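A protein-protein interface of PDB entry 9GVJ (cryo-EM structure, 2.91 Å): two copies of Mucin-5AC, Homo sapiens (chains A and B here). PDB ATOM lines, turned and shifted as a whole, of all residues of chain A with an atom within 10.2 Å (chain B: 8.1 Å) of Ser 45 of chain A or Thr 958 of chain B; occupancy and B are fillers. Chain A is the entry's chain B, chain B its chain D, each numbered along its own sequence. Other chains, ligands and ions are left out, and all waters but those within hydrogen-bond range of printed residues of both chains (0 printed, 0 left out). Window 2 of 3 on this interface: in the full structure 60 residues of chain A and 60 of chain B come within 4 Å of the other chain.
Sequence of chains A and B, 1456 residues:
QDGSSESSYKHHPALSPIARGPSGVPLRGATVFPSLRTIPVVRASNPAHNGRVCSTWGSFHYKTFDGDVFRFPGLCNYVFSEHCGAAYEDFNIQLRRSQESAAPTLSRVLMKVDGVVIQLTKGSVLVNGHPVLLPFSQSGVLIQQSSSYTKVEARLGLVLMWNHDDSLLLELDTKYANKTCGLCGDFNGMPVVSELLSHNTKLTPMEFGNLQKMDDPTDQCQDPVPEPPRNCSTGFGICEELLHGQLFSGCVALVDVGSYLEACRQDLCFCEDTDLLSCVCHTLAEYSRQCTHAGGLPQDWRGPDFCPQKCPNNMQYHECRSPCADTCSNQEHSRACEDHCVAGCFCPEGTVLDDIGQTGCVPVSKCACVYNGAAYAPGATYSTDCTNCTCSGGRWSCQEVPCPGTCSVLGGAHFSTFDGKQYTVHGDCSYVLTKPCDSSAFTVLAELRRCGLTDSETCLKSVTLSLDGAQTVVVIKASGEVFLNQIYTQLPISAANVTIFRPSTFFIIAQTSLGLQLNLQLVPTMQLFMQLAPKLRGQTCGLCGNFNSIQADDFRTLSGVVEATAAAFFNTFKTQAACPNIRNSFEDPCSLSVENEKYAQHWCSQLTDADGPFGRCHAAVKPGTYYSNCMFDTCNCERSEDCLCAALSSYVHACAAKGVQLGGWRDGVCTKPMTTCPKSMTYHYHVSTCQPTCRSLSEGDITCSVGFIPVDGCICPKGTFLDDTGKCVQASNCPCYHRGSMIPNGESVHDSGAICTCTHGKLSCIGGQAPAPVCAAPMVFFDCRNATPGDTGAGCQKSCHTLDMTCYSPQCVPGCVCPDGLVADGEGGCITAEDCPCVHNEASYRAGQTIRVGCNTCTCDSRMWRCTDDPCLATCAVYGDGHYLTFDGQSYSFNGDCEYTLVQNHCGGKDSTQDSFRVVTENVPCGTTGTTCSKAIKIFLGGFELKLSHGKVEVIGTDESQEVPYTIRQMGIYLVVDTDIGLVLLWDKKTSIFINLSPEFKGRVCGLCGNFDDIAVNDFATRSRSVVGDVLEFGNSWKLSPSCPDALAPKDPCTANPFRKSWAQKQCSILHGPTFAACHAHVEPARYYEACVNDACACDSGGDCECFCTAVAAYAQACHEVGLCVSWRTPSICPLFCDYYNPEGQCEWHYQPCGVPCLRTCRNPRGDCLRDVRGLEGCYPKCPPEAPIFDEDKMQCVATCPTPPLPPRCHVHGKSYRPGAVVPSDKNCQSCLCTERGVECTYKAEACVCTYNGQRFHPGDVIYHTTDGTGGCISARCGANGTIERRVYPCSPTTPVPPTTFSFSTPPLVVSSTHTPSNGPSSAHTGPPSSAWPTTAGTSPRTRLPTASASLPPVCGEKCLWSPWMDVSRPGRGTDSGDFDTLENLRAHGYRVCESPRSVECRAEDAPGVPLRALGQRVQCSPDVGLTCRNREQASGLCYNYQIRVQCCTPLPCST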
ATOM      1  N   VAL A  42      31.955 -17.559  10.260  1.00  0.00           N
ATOM      2  CA  VAL A  42      32.422 -17.780  11.624  1.00  0.00           C
ATOM      3  C   VAL A  42      32.035 -19.191  12.040  1.00  0.00           C
ATOM      4  O   VAL A  42      30.870 -19.587  11.908  1.00  0.00           O
ATOM      5  CB  VAL A  42      31.840 -16.740  12.596  1.00  0.00           C
ATOM      6  CG1 VAL A  42      32.424 -16.930  13.987  1.00  0.00           C
ATOM      7  CG2 VAL A  42      32.107 -15.331  12.087  1.00  0.00           C
ATOM      8  N   ARG A  43      33.008 -19.947  12.540  1.00  0.00           N
ATOM      9  CA  ARG A  43      32.804 -21.327  12.955  1.00  0.00           C
ATOM     10  C   ARG A  43      32.823 -21.426  14.474  1.00  0.00           C
ATOM     11  O   ARG A  43      33.653 -20.796  15.137  1.00  0.00           O
ATOM     12  CB  ARG A  43      33.874 -22.245  12.357  1.00  0.00           C
ATOM     13  CG  ARG A  43      33.575 -23.726  12.511  1.00  0.00           C
ATOM     14  CD  ARG A  43      33.836 -24.485  11.217  1.00  0.00           C
ATOM     15  NE  ARG A  43      34.210 -25.875  11.458  1.00  0.00           N
ATOM     16  CZ  ARG A  43      33.382 -26.817  11.888  1.00  0.00           C
ATOM     17  NH1 ARG A  43      32.104 -26.562  12.122  1.00  0.00           N
ATOM     18  NH2 ARG A  43      33.846 -28.048  12.085  1.00  0.00           N
ATOM     19  N   ALA A  44      31.903 -22.220  15.018  1.00  0.00           N
ATOM     20  CA  ALA A  44      31.817 -22.430  16.460  1.00  0.00           C
ATOM     21  C   ALA A  44      31.286 -23.837  16.694  1.00  0.00           C
ATOM     22  O   ALA A  44      30.129 -24.124  16.372  1.00  0.00           O
ATOM     23  CB  ALA A  44      30.922 -21.385  17.119  1.00  0.00           C
ATOM     24  N   SER A  45      32.128 -24.709  17.249  1.00  0.00           N
ATOM     25  CA  SER A  45      31.768 -26.104  17.472  1.00  0.00           C
ATOM     26  C   SER A  45      31.886 -26.517  18.934  1.00  0.00           C
ATOM     27  O   SER A  45      31.768 -27.709  19.240  1.00  0.00           O
ATOM     28  CB  SER A  45      32.633 -27.020  16.602  1.00  0.00           C
ATOM     29  OG  SER A  45      34.011 -26.793  16.835  1.00  0.00           O
ATOM     30  N   ASN A  46      32.114 -25.569  19.844  1.00  0.00           N
ATOM     31  CA  ASN A  46      32.248 -25.889  21.258  1.00  0.00           C
ATOM     32  C   ASN A  46      30.948 -25.558  21.973  1.00  0.00           C
ATOM     33  O   ASN A  46      30.607 -24.372  22.097  1.00  0.00           O
ATOM     34  CB  ASN A  46      33.410 -25.115  21.875  1.00  0.00           C
ATOM     35  CG  ASN A  46      33.599 -25.424  23.347  1.00  0.00           C
ATOM     36  OD1 ASN A  46      33.872 -24.533  24.150  1.00  0.00           O
ATOM     37  ND2 ASN A  46      33.455 -26.694  23.708  1.00  0.00           N
ATOM     38  N   PRO A  47      30.192 -26.552  22.449  1.00  0.00           N
ATOM     39  CA  PRO A  47      28.917 -26.249  23.121  1.00  0.00           C
ATOM     40  C   PRO A  47      29.071 -25.473  24.417  1.00  0.00           C
ATOM     41  O   PRO A  47      28.116 -24.811  24.838  1.00  0.00           O
ATOM     42  CB  PRO A  47      28.315 -27.639  23.366  1.00  0.00           C
ATOM     43  CG  PRO A  47      29.495 -28.554  23.407  1.00  0.00           C
ATOM     44  CD  PRO A  47      30.470 -27.996  22.409  1.00  0.00           C
ATOM     45  N   ALA A  48      30.233 -25.535  25.066  1.00  0.00           N
ATOM     46  CA  ALA A  48      30.451 -24.810  26.315  1.00  0.00           C
ATOM     47  C   ALA A  48      30.439 -23.313  26.035  1.00  0.00           C
ATOM     48  O   ALA A  48      31.360 -22.783  25.405  1.00  0.00           O
ATOM     49  CB  ALA A  48      31.768 -25.239  26.954  1.00  0.00           C
ATOM     50  N   HIS A  49      29.399 -22.628  26.504  1.00  0.00           N
ATOM     51  CA  HIS A  49      29.202 -21.213  26.208  1.00  0.00           C
ATOM     52  C   HIS A  49      28.793 -20.450  27.459  1.00  0.00           C
ATOM     53  O   HIS A  49      27.911 -19.586  27.421  1.00  0.00           O
ATOM     54  CB  HIS A  49      28.170 -21.027  25.097  1.00  0.00           C
ATOM     55  CG  HIS A  49      26.850 -21.673  25.383  1.00  0.00           C
ATOM     56  ND1 HIS A  49      26.527 -22.934  24.927  1.00  0.00           N
ATOM     57  CD2 HIS A  49      25.770 -21.235  26.072  1.00  0.00           C
ATOM     58  CE1 HIS A  49      25.308 -23.245  25.328  1.00  0.00           C
ATOM     59  NE2 HIS A  49      24.826 -22.231  26.023  1.00  0.00           N
ATOM     60  N   ARG A  52      28.974 -16.466  27.372  1.00  0.00           N
ATOM     61  CA  ARG A  52      27.911 -15.622  26.849  1.00  0.00           C
ATOM     62  C   ARG A  52      26.727 -15.520  27.800  1.00  0.00           C
ATOM     63  O   ARG A  52      25.675 -15.003  27.412  1.00  0.00           O
ATOM     64  CB  ARG A  52      27.439 -16.147  25.491  1.00  0.00           C
ATOM     65  CG  ARG A  52      28.562 -16.462  24.518  1.00  0.00           C
ATOM     66  CD  ARG A  52      28.042 -17.230  23.313  1.00  0.00           C
ATOM     67  NE  ARG A  52      26.599 -17.081  23.156  1.00  0.00           N
ATOM     68  CZ  ARG A  52      25.751 -18.091  23.024  1.00  0.00           C
ATOM     69  NH1 ARG A  52      26.167 -19.347  23.014  1.00  0.00           N
ATOM     70  NH2 ARG A  52      24.452 -17.835  22.895  1.00  0.00           N
ATOM     71  N   THR A 174      27.247 -13.540  20.508  1.00  0.00           N
ATOM     72  CA  THR A 174      28.683 -13.288  20.453  1.00  0.00           C
ATOM     73  C   THR A 174      29.004 -11.968  19.761  1.00  0.00           C
ATOM     74  O   THR A 174      30.105 -11.436  19.939  1.00  0.00           O
ATOM     75  CB  THR A 174      29.385 -14.449  19.742  1.00  0.00           C
ATOM     76  OG1 THR A 174      28.904 -15.690  20.272  1.00  0.00           O
ATOM     77  CG2 THR A 174      30.893 -14.385  19.948  1.00  0.00           C
ATOM     78  N   ALA A 294      27.011 -25.205  29.856  1.00  0.00           N
ATOM     79  CA  ALA A 294      28.368 -25.615  29.524  1.00  0.00           C
ATOM     80  C   ALA A 294      28.415 -26.872  28.667  1.00  0.00           C
ATOM     81  O   ALA A 294      29.506 -27.389  28.407  1.00  0.00           O
ATOM     82  CB  ALA A 294      29.181 -25.834  30.802  1.00  0.00           C
ATOM     83  N   GLY A 295      27.266 -27.372  28.223  1.00  0.00           N
ATOM     84  CA  GLY A 295      27.212 -28.594  27.450  1.00  0.00           C
ATOM     85  C   GLY A 295      27.138 -29.867  28.260  1.00  0.00           C
ATOM     86  O   GLY A 295      27.192 -30.955  27.676  1.00  0.00           O
ATOM     87  N   LEU B 941      21.593 -29.820   8.410  1.00  0.00           N
ATOM     88  CA  LEU B 941      21.673 -31.176   7.885  1.00  0.00           C
ATOM     89  C   LEU B 941      22.901 -31.855   8.470  1.00  0.00           C
ATOM     90  O   LEU B 941      23.882 -31.198   8.831  1.00  0.00           O
ATOM     91  CB  LEU B 941      21.699 -31.229   6.350  1.00  0.00           C
ATOM     92  CG  LEU B 941      22.999 -31.121   5.557  1.00  0.00           C
ATOM     93  CD1 LEU B 941      22.740 -31.444   4.098  1.00  0.00           C
ATOM     94  CD2 LEU B 941      23.553 -29.736   5.671  1.00  0.00           C
ATOM     95  N   GLY B 942      22.834 -33.182   8.554  1.00  0.00           N
ATOM     96  CA  GLY B 942      23.836 -33.905   9.313  1.00  0.00           C
ATOM     97  C   GLY B 942      23.818 -33.446  10.755  1.00  0.00           C
ATOM     98  O   GLY B 942      22.759 -33.295  11.374  1.00  0.00           O
ATOM     99  N   GLY B 943      25.005 -33.218  11.303  1.00  0.00           N
ATOM    100  CA  GLY B 943      25.112 -32.601  12.609  1.00  0.00           C
ATOM    101  C   GLY B 943      25.479 -31.137  12.492  1.00  0.00           C
ATOM    102  O   GLY B 943      25.939 -30.525  13.460  1.00  0.00           O
ATOM    103  N   PHE B 944      25.278 -30.566  11.308  1.00  0.00           N
ATOM    104  CA  PHE B 944      25.796 -29.247  10.975  1.00  0.00           C
ATOM    105  C   PHE B 944      24.665 -28.250  10.754  1.00  0.00           C
ATOM    106  O   PHE B 944      23.617 -28.588  10.187  1.00  0.00           O
ATOM    107  CB  PHE B 944      26.687 -29.319   9.734  1.00  0.00           C
ATOM    108  CG  PHE B 944      28.066 -29.844  10.012  1.00  0.00           C
ATOM    109  CD1 PHE B 944      28.735 -30.604   9.071  1.00  0.00           C
ATOM    110  CD2 PHE B 944      28.692 -29.576  11.215  1.00  0.00           C
ATOM    111  CE1 PHE B 944      30.002 -31.088   9.326  1.00  0.00           C
ATOM    112  CE2 PHE B 944      29.959 -30.055  11.476  1.00  0.00           C
ATOM    113  CZ  PHE B 944      30.615 -30.813  10.531  1.00  0.00           C
ATOM    114  N   GLU B 945      24.894 -27.018  11.214  1.00  0.00           N
ATOM    115  CA  GLU B 945      23.933 -25.928  11.126  1.00  0.00           C
ATOM    116  C   GLU B 945      24.620 -24.671  10.612  1.00  0.00           C
ATOM    117  O   GLU B 945      25.681 -24.289  11.118  1.00  0.00           O
ATOM    118  CB  GLU B 945      23.299 -25.640  12.491  1.00  0.00           C
ATOM    119  CG  GLU B 945      22.716 -24.240  12.611  1.00  0.00           C
ATOM    120  CD  GLU B 945      22.298 -23.896  14.027  1.00  0.00           C
ATOM    121  OE1 GLU B 945      22.489 -24.742  14.925  1.00  0.00           O
ATOM    122  OE2 GLU B 945      21.779 -22.781  14.240  1.00  0.00           O
ATOM    123  N   VAL B 955      28.674 -20.871  11.344  1.00  0.00           N
ATOM    124  CA  VAL B 955      28.661 -22.329  11.344  1.00  0.00           C
ATOM    125  C   VAL B 955      28.632 -22.782  12.796  1.00  0.00           C
ATOM    126  O   VAL B 955      29.642 -22.699  13.505  1.00  0.00           O
ATOM    127  CB  VAL B 955      29.869 -22.908  10.597  1.00  0.00           C
ATOM    128  CG1 VAL B 955      29.851 -24.426  10.665  1.00  0.00           C
ATOM    129  CG2 VAL B 955      29.872 -22.435   9.152  1.00  0.00           C
ATOM    130  N   ILE B 956      27.475 -23.267  13.244  1.00  0.00           N
ATOM    131  CA  ILE B 956      27.298 -23.672  14.634  1.00  0.00           C
ATOM    132  C   ILE B 956      27.223 -25.194  14.669  1.00  0.00           C
ATOM    133  O   ILE B 956      26.651 -25.788  15.590  1.00  0.00           O
ATOM    134  CB  ILE B 956      26.046 -23.013  15.244  1.00  0.00           C
ATOM    135  CG1 ILE B 956      26.015 -21.527  14.889  1.00  0.00           C
ATOM    136  CG2 ILE B 956      26.060 -23.112  16.763  1.00  0.00           C
ATOM    137  CD1 ILE B 956      24.699 -21.070  14.300  1.00  0.00           C
ATOM    138  N   GLY B 957      27.806 -25.837  13.661  1.00  0.00           N
ATOM    139  CA  GLY B 957      27.815 -27.280  13.589  1.00  0.00           C
ATOM    140  C   GLY B 957      28.889 -27.902  14.460  1.00  0.00           C
ATOM    141  O   GLY B 957      29.723 -27.225  15.061  1.00  0.00           O
ATOM    142  N   THR B 958      28.853 -29.233  14.518  1.00  0.00           N
ATOM    143  CA  THR B 958      29.789 -30.027  15.317  1.00  0.00           C
ATOM    144  C   THR B 958      29.788 -29.600  16.781  1.00  0.00           C
ATOM    145  O   THR B 958      30.401 -30.252  17.627  1.00  0.00           O
ATOM    146  CB  THR B 958      31.228 -29.939  14.768  1.00  0.00           C
ATOM    147  N   GLN B 962      32.419 -36.730  10.512  1.00  0.00           N
ATOM    148  CA  GLN B 962      32.284 -36.363   9.107  1.00  0.00           C
ATOM    149  C   GLN B 962      32.776 -34.939   8.870  1.00  0.00           C
ATOM    150  O   GLN B 962      32.806 -34.122   9.790  1.00  0.00           O
ATOM    151  CB  GLN B 962      30.830 -36.504   8.654  1.00  0.00           C
ATOM    152  CG  GLN B 962      30.334 -37.940   8.609  1.00  0.00           C
ATOM    153  CD  GLN B 962      28.863 -38.038   8.256  1.00  0.00           C
ATOM    154  OE1 GLN B 962      28.093 -37.106   8.488  1.00  0.00           O
ATOM    155  NE2 GLN B 962      28.465 -39.173   7.692  1.00  0.00           N
ATOM    156  N   VAL B 964      32.807 -31.232   6.390  1.00  0.00           N
ATOM    157  CA  VAL B 964      31.821 -30.179   6.164  1.00  0.00           C
ATOM    158  C   VAL B 964      31.236 -30.372   4.765  1.00  0.00           C
ATOM    159  O   VAL B 964      31.970 -30.215   3.775  1.00  0.00           O
ATOM    160  CB  VAL B 964      32.454 -28.790   6.314  1.00  0.00           C
ATOM    161  CG1 VAL B 964      31.443 -27.707   6.018  1.00  0.00           C
ATOM    162  CG2 VAL B 964      33.021 -28.619   7.715  1.00  0.00           C
ATOM    163  N   TYR B 966      29.485 -28.409   2.874  1.00  0.00           N
ATOM    164  CA  TYR B 966      29.034 -27.066   2.549  1.00  0.00           C
ATOM    165  C   TYR B 966      29.995 -26.427   1.560  1.00  0.00           C
ATOM    166  O   TYR B 966      31.175 -26.782   1.497  1.00  0.00           O
ATOM    167  CB  TYR B 966      28.940 -26.190   3.802  1.00  0.00           C
ATOM    168  CG  TYR B 966      27.837 -26.572   4.761  1.00  0.00           C
ATOM    169  CD1 TYR B 966      26.501 -26.476   4.395  1.00  0.00           C
ATOM    170  CD2 TYR B 966      28.134 -27.050   6.028  1.00  0.00           C
ATOM    171  CE1 TYR B 966      25.495 -26.824   5.279  1.00  0.00           C
ATOM    172  CE2 TYR B 966      27.144 -27.413   6.906  1.00  0.00           C
ATOM    173  CZ  TYR B 966      25.826 -27.295   6.534  1.00  0.00           C
ATOM    174  OH  TYR B 966      24.845 -27.646   7.429  1.00  0.00           O
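The backbone carbonyl oxygen of Gly 943 of chain B sits at hydrogen-bond distance from the backbone NH of Thr 958 of chain B (3.4 Å). O of Glu 945 of chain B is in hydrogen-bond range of N of Ile 956 of chain B.
Printed residues of chain A that touch a printed residue of chain B: Val 42, Arg 43, Ala 44 and Ser 45. Printed residues of chain B that touch a printed residue of chain A: Val 955, Ile 956, Gly 957 and Thr 958.
O of Val 42 of chain A sits at hydrogen-bond distance from N of Val 955 of chain B, 2.6 Å away. N of Ala 44 of chain A is in hydrogen-bond range of O of Val 955 of chain B. The backbone carbonyl oxygen (O) of Ala 44 of chain A lies close to the backbone carbonyl oxygen (O) of Gly 957 of chain B. O of Ser 45 of chain A lies close to O of Thr 958 of chain B (3.3 Å).
Arg 43 of chain A touches Val 955 of chain B. Gly 957 of chain B touches Arg 43 of chain A (O to NH1, 3.8 Å). CA of Ile 956 of chain B touches O of Ala 44 of chain A, 3.4 Å away. Ser 45 of chain A touches Gly 957 of chain B (CB to O, 3.3 Å).
No position is printed for both chains. Of the 8 pairs that touch across the chains among the printed residues, none has its exchanged pair printed and touching as well.
Ser 45 of chain A touches just these residues of chain B: Gly 957 (3.3 Å) and Thr 958 (3.3 Å). Of chain A, only Ser 45 comes within 4 Å of Thr 958 of chain B. Ala 44 of chain A touches just these residues of chain B: Val 955 (2.8 Å), Ile 956 (3.4 Å) and Gly 957 (3.4 Å). Gly 957 of chain B touches three residues of chain A. Printed residues of chain A within 4 Å of Ile 956 of chain B: Ala 44 (3.4 Å). Of the printed residues of chain B, Arg 43 of chain A touches Val 955 (3.4 Å) and Gly 957 (3.8 Å). Of the printed residues of chain B, Val 42 of chain A touches Val 955 (2.6 Å). Gly 295 of chain A touches none of the printed residues of chain B. The nearest printed residue of chain A that does not touch Ile 956 of chain B is Val 42 of chain A (5.2 Å).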
